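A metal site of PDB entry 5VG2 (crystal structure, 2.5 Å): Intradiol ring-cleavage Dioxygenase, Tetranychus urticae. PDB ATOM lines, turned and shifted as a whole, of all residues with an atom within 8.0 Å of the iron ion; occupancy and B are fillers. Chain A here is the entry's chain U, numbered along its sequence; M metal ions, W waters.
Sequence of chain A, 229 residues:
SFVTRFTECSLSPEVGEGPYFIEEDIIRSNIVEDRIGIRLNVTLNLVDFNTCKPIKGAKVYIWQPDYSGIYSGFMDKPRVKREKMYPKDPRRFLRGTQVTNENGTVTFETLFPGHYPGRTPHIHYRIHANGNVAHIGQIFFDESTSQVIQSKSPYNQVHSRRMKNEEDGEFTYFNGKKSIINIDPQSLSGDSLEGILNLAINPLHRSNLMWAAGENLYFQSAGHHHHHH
The iron ion is bound by the side-chain hydroxyl (OH) of Tyr 71 (1.9 Å), water W1 (2.0 Å), a ring nitrogen (NE2) of His 124 (2.2 Å), a ring nitrogen (NE2) of His 122 (2.3 Å) and the side-chain hydroxyl (OH) of Tyr 116 (2.5 Å). The iron ion has five donor atoms within binding distance.
The backbone NH (N) of His 124 is in hydrogen-bond range of the backbone carbonyl oxygen (O) of Trp 63 (3.0 Å). A ring nitrogen (ND1) of His 124 sits at hydrogen-bond distance from the backbone carbonyl oxygen (O) of Glu 17. The backbone carbonyl oxygen (O) of Thr 120 lies within hydrogen-bond range of a ring nitrogen (ND1) of His 122 (2.7 Å).
Along chain A the residues within 4 Å of the iron ion span positions 71 to 124. The nearest printed residue that does not touch the iron ion is Arg 119 (4.1 Å).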
ATOM      1  N   GLY A  16       4.958  -3.165  29.946  1.00  0.00           N
ATOM      2  CA  GLY A  16       5.029  -4.090  31.087  1.00  0.00           C
ATOM      3  C   GLY A  16       4.605  -5.503  30.727  1.00  0.00           C
ATOM      4  O   GLY A  16       3.704  -5.719  29.902  1.00  0.00           O
ATOM      5  N   GLU A  17       5.290  -6.467  31.308  1.00  0.00           N
ATOM      6  CA  GLU A  17       5.035  -7.868  31.014  1.00  0.00           C
ATOM      7  C   GLU A  17       3.635  -8.323  31.502  1.00  0.00           C
ATOM      8  O   GLU A  17       3.010  -9.229  30.952  1.00  0.00           O
ATOM      9  CB  GLU A  17       6.107  -8.667  31.701  1.00  0.00           C
ATOM     10  CG  GLU A  17       6.058 -10.159  31.505  1.00  0.00           C
ATOM     11  CD  GLU A  17       7.321 -10.833  32.055  1.00  0.00           C
ATOM     12  OE1 GLU A  17       7.373 -11.114  33.277  1.00  0.00           O
ATOM     13  OE2 GLU A  17       8.273 -11.084  31.272  1.00  0.00           O
ATOM     14  N   GLY A  18       3.160  -7.697  32.557  1.00  0.00           N
ATOM     15  CA  GLY A  18       2.034  -8.204  33.296  1.00  0.00           C
ATOM     16  C   GLY A  18       2.401  -9.443  34.079  1.00  0.00           C
ATOM     17  O   GLY A  18       3.532  -9.889  34.084  1.00  0.00           O
ATOM     18  N   PRO A  19       1.419 -10.038  34.767  1.00  0.00           N
ATOM     19  CA  PRO A  19       1.746 -11.101  35.694  1.00  0.00           C
ATOM     20  C   PRO A  19       1.707 -12.519  35.117  1.00  0.00           C
ATOM     21  O   PRO A  19       1.893 -13.440  35.908  1.00  0.00           O
ATOM     22  CB  PRO A  19       0.694 -10.919  36.779  1.00  0.00           C
ATOM     23  CG  PRO A  19      -0.508 -10.334  36.058  1.00  0.00           C
ATOM     24  CD  PRO A  19       0.031  -9.523  34.910  1.00  0.00           C
ATOM     25  N   TYR A  20       1.511 -12.711  33.806  1.00  0.00           N
ATOM     26  CA  TYR A  20       1.217 -14.075  33.287  1.00  0.00           C
ATOM     27  C   TYR A  20       2.188 -14.710  32.308  1.00  0.00           C
ATOM     28  O   TYR A  20       1.842 -15.645  31.596  1.00  0.00           O
ATOM     29  CB  TYR A  20      -0.169 -14.116  32.645  1.00  0.00           C
ATOM     30  CG  TYR A  20      -1.266 -13.664  33.521  1.00  0.00           C
ATOM     31  CD1 TYR A  20      -1.505 -14.258  34.764  1.00  0.00           C
ATOM     32  CD2 TYR A  20      -2.140 -12.675  33.087  1.00  0.00           C
ATOM     33  CE1 TYR A  20      -2.576 -13.852  35.573  1.00  0.00           C
ATOM     34  CE2 TYR A  20      -3.231 -12.268  33.869  1.00  0.00           C
ATOM     35  CZ  TYR A  20      -3.441 -12.858  35.102  1.00  0.00           C
ATOM     36  OH  TYR A  20      -4.515 -12.444  35.845  1.00  0.00           O
ATOM     37  N   PHE A  21       3.390 -14.188  32.236  1.00  0.00           N
ATOM     38  CA  PHE A  21       4.421 -14.892  31.530  1.00  0.00           C
ATOM     39  C   PHE A  21       4.778 -16.220  32.217  1.00  0.00           C
ATOM     40  O   PHE A  21       4.809 -16.297  33.401  1.00  0.00           O
ATOM     41  CB  PHE A  21       5.662 -14.009  31.409  1.00  0.00           C
ATOM     42  CG  PHE A  21       6.719 -14.616  30.537  1.00  0.00           C
ATOM     43  CD1 PHE A  21       6.425 -14.941  29.228  1.00  0.00           C
ATOM     44  CD2 PHE A  21       7.980 -14.911  31.051  1.00  0.00           C
ATOM     45  CE1 PHE A  21       7.383 -15.521  28.421  1.00  0.00           C
ATOM     46  CE2 PHE A  21       8.928 -15.493  30.247  1.00  0.00           C
ATOM     47  CZ  PHE A  21       8.637 -15.781  28.930  1.00  0.00           C
ATOM     48  N   TRP A  63       2.265 -14.579  24.397  1.00  0.00           N
ATOM     49  CA  TRP A  63       1.163 -15.149  25.179  1.00  0.00           C
ATOM     50  C   TRP A  63       0.033 -14.202  25.135  1.00  0.00           C
ATOM     51  O   TRP A  63       0.237 -13.027  24.935  1.00  0.00           O
ATOM     52  CB  TRP A  63       1.589 -15.505  26.626  1.00  0.00           C
ATOM     53  CG  TRP A  63       1.947 -14.398  27.541  1.00  0.00           C
ATOM     54  CD1 TRP A  63       1.249 -13.976  28.640  1.00  0.00           C
ATOM     55  CD2 TRP A  63       3.141 -13.624  27.518  1.00  0.00           C
ATOM     56  NE1 TRP A  63       1.915 -12.950  29.263  1.00  0.00           N
ATOM     57  CE2 TRP A  63       3.078 -12.713  28.584  1.00  0.00           C
ATOM     58  CE3 TRP A  63       4.245 -13.596  26.672  1.00  0.00           C
ATOM     59  CZ2 TRP A  63       4.068 -11.767  28.817  1.00  0.00           C
ATOM     60  CZ3 TRP A  63       5.265 -12.650  26.928  1.00  0.00           C
ATOM     61  CH2 TRP A  63       5.163 -11.767  27.962  1.00  0.00           C
ATOM     62  N   GLN A  64      -1.180 -14.737  25.263  1.00  0.00           N
ATOM     63  CA  GLN A  64      -2.359 -13.938  25.135  1.00  0.00           C
ATOM     64  C   GLN A  64      -3.534 -14.693  25.722  1.00  0.00           C
ATOM     65  O   GLN A  64      -3.496 -15.903  25.772  1.00  0.00           O
ATOM     66  CB  GLN A  64      -2.635 -13.657  23.629  1.00  0.00           C
ATOM     67  CG  GLN A  64      -3.225 -14.836  22.881  1.00  0.00           C
ATOM     68  CD  GLN A  64      -3.387 -14.610  21.373  1.00  0.00           C
ATOM     69  OE1 GLN A  64      -2.397 -14.525  20.623  1.00  0.00           O
ATOM     70  NE2 GLN A  64      -4.652 -14.595  20.919  1.00  0.00           N
ATOM     71  N   PRO A  65      -4.581 -13.986  26.132  1.00  0.00           N
ATOM     72  CA  PRO A  65      -5.770 -14.622  26.697  1.00  0.00           C
ATOM     73  C   PRO A  65      -6.675 -15.158  25.633  1.00  0.00           C
ATOM     74  O   PRO A  65      -6.639 -14.724  24.481  1.00  0.00           O
ATOM     75  CB  PRO A  65      -6.475 -13.468  27.420  1.00  0.00           C
ATOM     76  CG  PRO A  65      -6.099 -12.271  26.609  1.00  0.00           C
ATOM     77  CD  PRO A  65      -4.700 -12.517  26.140  1.00  0.00           C
ATOM     78  N   GLY A  69     -11.043 -14.016  27.895  1.00  0.00           N
ATOM     79  CA  GLY A  69     -10.078 -13.314  28.764  1.00  0.00           C
ATOM     80  C   GLY A  69      -9.294 -14.211  29.723  1.00  0.00           C
ATOM     81  O   GLY A  69      -8.799 -13.748  30.744  1.00  0.00           O
ATOM     82  N   TYR A  71      -6.041 -16.690  30.583  1.00  0.00           N
ATOM     83  CA  TYR A  71      -4.703 -17.168  30.337  1.00  0.00           C
ATOM     84  C   TYR A  71      -4.500 -18.602  30.780  1.00  0.00           C
ATOM     85  O   TYR A  71      -4.901 -18.959  31.893  1.00  0.00           O
ATOM     86  CB  TYR A  71      -3.708 -16.301  31.083  1.00  0.00           C
ATOM     87  CG  TYR A  71      -3.537 -14.918  30.499  1.00  0.00           C
ATOM     88  CD1 TYR A  71      -2.651 -14.703  29.465  1.00  0.00           C
ATOM     89  CD2 TYR A  71      -4.276 -13.845  30.964  1.00  0.00           C
ATOM     90  CE1 TYR A  71      -2.485 -13.451  28.906  1.00  0.00           C
ATOM     91  CE2 TYR A  71      -4.126 -12.578  30.395  1.00  0.00           C
ATOM     92  CZ  TYR A  71      -3.202 -12.398  29.364  1.00  0.00           C
ATOM     93  OH  TYR A  71      -2.920 -11.166  28.795  1.00  0.00           O
ATOM     94  N   GLY A 114      -8.929 -12.109  23.315  1.00  0.00           N
ATOM     95  CA  GLY A 114     -10.090 -11.627  24.079  1.00  0.00           C
ATOM     96  C   GLY A 114      -9.659 -10.443  24.894  1.00  0.00           C
ATOM     97  O   GLY A 114      -8.484 -10.185  25.040  1.00  0.00           O
ATOM     98  N   TYR A 116     -10.293  -8.659  28.774  1.00  0.00           N
ATOM     99  CA  TYR A 116     -10.786  -8.914  30.100  1.00  0.00           C
ATOM    100  C   TYR A 116     -10.972  -7.590  30.819  1.00  0.00           C
ATOM    101  O   TYR A 116     -10.499  -6.569  30.346  1.00  0.00           O
ATOM    102  CB  TYR A 116      -9.880  -9.872  30.829  1.00  0.00           C
ATOM    103  CG  TYR A 116      -8.420  -9.562  30.801  1.00  0.00           C
ATOM    104  CD1 TYR A 116      -7.635  -9.962  29.748  1.00  0.00           C
ATOM    105  CD2 TYR A 116      -7.829  -8.881  31.848  1.00  0.00           C
ATOM    106  CE1 TYR A 116      -6.250  -9.739  29.746  1.00  0.00           C
ATOM    107  CE2 TYR A 116      -6.478  -8.617  31.855  1.00  0.00           C
ATOM    108  CZ  TYR A 116      -5.690  -9.049  30.798  1.00  0.00           C
ATOM    109  OH  TYR A 116      -4.380  -8.778  30.814  1.00  0.00           O
ATOM    110  N   ARG A 119      -8.675  -4.142  30.604  1.00  0.00           N
ATOM    111  CA  ARG A 119      -7.696  -4.171  29.525  1.00  0.00           C
ATOM    112  C   ARG A 119      -8.321  -4.214  28.140  1.00  0.00           C
ATOM    113  O   ARG A 119      -9.322  -4.855  27.912  1.00  0.00           O
ATOM    114  CB  ARG A 119      -6.725  -5.353  29.632  1.00  0.00           C
ATOM    115  CG  ARG A 119      -5.844  -5.396  30.886  1.00  0.00           C
ATOM    116  CD  ARG A 119      -4.798  -4.308  30.997  1.00  0.00           C
ATOM    117  NE  ARG A 119      -4.292  -3.829  29.709  1.00  0.00           N
ATOM    118  CZ  ARG A 119      -3.227  -4.320  29.064  1.00  0.00           C
ATOM    119  NH1 ARG A 119      -2.871  -3.794  27.918  1.00  0.00           N
ATOM    120  NH2 ARG A 119      -2.545  -5.350  29.545  1.00  0.00           N
ATOM    121  N   THR A 120      -7.689  -3.483  27.235  1.00  0.00           N
ATOM    122  CA  THR A 120      -7.952  -3.565  25.803  1.00  0.00           C
ATOM    123  C   THR A 120      -7.400  -4.879  25.221  1.00  0.00           C
ATOM    124  O   THR A 120      -6.460  -5.441  25.778  1.00  0.00           O
ATOM    125  CB  THR A 120      -7.373  -2.314  25.111  1.00  0.00           C
ATOM    126  OG1 THR A 120      -7.913  -2.204  23.820  1.00  0.00           O
ATOM    127  CG2 THR A 120      -5.841  -2.351  25.024  1.00  0.00           C
ATOM    128  N   PRO A 121      -7.950  -5.360  24.097  1.00  0.00           N
ATOM    129  CA  PRO A 121      -7.329  -6.556  23.518  1.00  0.00           C
ATOM    130  C   PRO A 121      -5.858  -6.347  23.135  1.00  0.00           C
ATOM    131  O   PRO A 121      -5.493  -5.315  22.664  1.00  0.00           O
ATOM    132  CB  PRO A 121      -8.202  -6.877  22.294  1.00  0.00           C
ATOM    133  CG  PRO A 121      -9.455  -6.108  22.499  1.00  0.00           C
ATOM    134  CD  PRO A 121      -9.046  -4.869  23.242  1.00  0.00           C
ATOM    135  N   HIS A 122      -5.035  -7.351  23.384  1.00  0.00           N
ATOM    136  CA  HIS A 122      -3.601  -7.271  23.214  1.00  0.00           C
ATOM    137  C   HIS A 122      -2.976  -8.645  23.197  1.00  0.00           C
ATOM    138  O   HIS A 122      -3.569  -9.598  23.692  1.00  0.00           O
ATOM    139  CB  HIS A 122      -2.969  -6.502  24.355  1.00  0.00           C
ATOM    140  CG  HIS A 122      -3.179  -7.122  25.703  1.00  0.00           C
ATOM    141  ND1 HIS A 122      -4.312  -6.885  26.448  1.00  0.00           N
ATOM    142  CD2 HIS A 122      -2.416  -7.989  26.427  1.00  0.00           C
ATOM    143  CE1 HIS A 122      -4.222  -7.568  27.587  1.00  0.00           C
ATOM    144  NE2 HIS A 122      -3.091  -8.245  27.592  1.00  0.00           N
ATOM    145  N   ILE A 123      -1.764  -8.715  22.661  1.00  0.00           N
ATOM    146  CA  ILE A 123      -0.944  -9.880  22.709  1.00  0.00           C
ATOM    147  C   ILE A 123       0.380  -9.436  23.337  1.00  0.00           C
ATOM    148  O   ILE A 123       0.947  -8.438  22.910  1.00  0.00           O
ATOM    149  CB  ILE A 123      -0.643 -10.422  21.305  1.00  0.00           C
ATOM    150  CG1 ILE A 123      -1.907 -10.920  20.674  1.00  0.00           C
ATOM    151  CG2 ILE A 123       0.393 -11.554  21.373  1.00  0.00           C
ATOM    152  CD1 ILE A 123      -1.740 -11.306  19.221  1.00  0.00           C
ATOM    153  N   HIS A 124       0.873 -10.194  24.314  1.00  0.00           N
ATOM    154  CA  HIS A 124       2.122  -9.924  24.963  1.00  0.00           C
ATOM    155  C   HIS A 124       3.271 -10.594  24.178  1.00  0.00           C
ATOM    156  O   HIS A 124       3.121 -11.675  23.636  1.00  0.00           O
ATOM    157  CB  HIS A 124       2.166 -10.575  26.323  1.00  0.00           C
ATOM    158  CG  HIS A 124       1.231  -9.994  27.322  1.00  0.00           C
ATOM    159  ND1 HIS A 124       1.553  -8.930  28.114  1.00  0.00           N
ATOM    160  CD2 HIS A 124       0.001 -10.376  27.716  1.00  0.00           C
ATOM    161  CE1 HIS A 124       0.552  -8.646  28.921  1.00  0.00           C
ATOM    162  NE2 HIS A 124      -0.394  -9.509  28.697  1.00  0.00           N
ATOM    163  N   GLN A 138       3.808  -5.258  24.020  1.00  0.00           N
ATOM    164  CA  GLN A 138       2.468  -5.690  23.755  1.00  0.00           C
ATOM    165  C   GLN A 138       2.056  -5.219  22.367  1.00  0.00           C
ATOM    166  O   GLN A 138       2.433  -4.162  21.938  1.00  0.00           O
ATOM    167  CB  GLN A 138       1.506  -5.166  24.808  1.00  0.00           C
ATOM    168  CG  GLN A 138       1.767  -5.704  26.226  1.00  0.00           C
ATOM    169  CD  GLN A 138       0.709  -5.272  27.241  1.00  0.00           C
ATOM    170  OE1 GLN A 138      -0.365  -4.844  26.864  1.00  0.00           O
ATOM    171  NE2 GLN A 138       1.008  -5.390  28.508  1.00  0.00           N
ATOM    172  N   GLU A 170      -2.022   0.758  30.228  1.00  0.00           N
ATOM    173  CA  GLU A 170      -0.760   0.324  29.623  1.00  0.00           C
ATOM    174  C   GLU A 170      -0.525   0.929  28.281  1.00  0.00           C
ATOM    175  O   GLU A 170       0.591   1.359  27.979  1.00  0.00           O
ATOM    176  CB  GLU A 170      -0.636  -1.213  29.664  1.00  0.00           C
ATOM    177  CG  GLU A 170      -0.279  -1.573  31.125  1.00  0.00           C
ATOM    178  CD  GLU A 170      -0.693  -2.970  31.553  1.00  0.00           C
ATOM    179  OE1 GLU A 170      -0.112  -3.932  31.016  1.00  0.00           O
ATOM    180  OE2 GLU A 170      -1.512  -3.087  32.512  1.00  0.00           O
HETATM  181 FE    FE M   1      -2.409  -9.466  29.463  1.00  0.00          FE
HETATM  182  O   HOH W   1      -2.099  -7.852  30.665  1.00  0.00           O
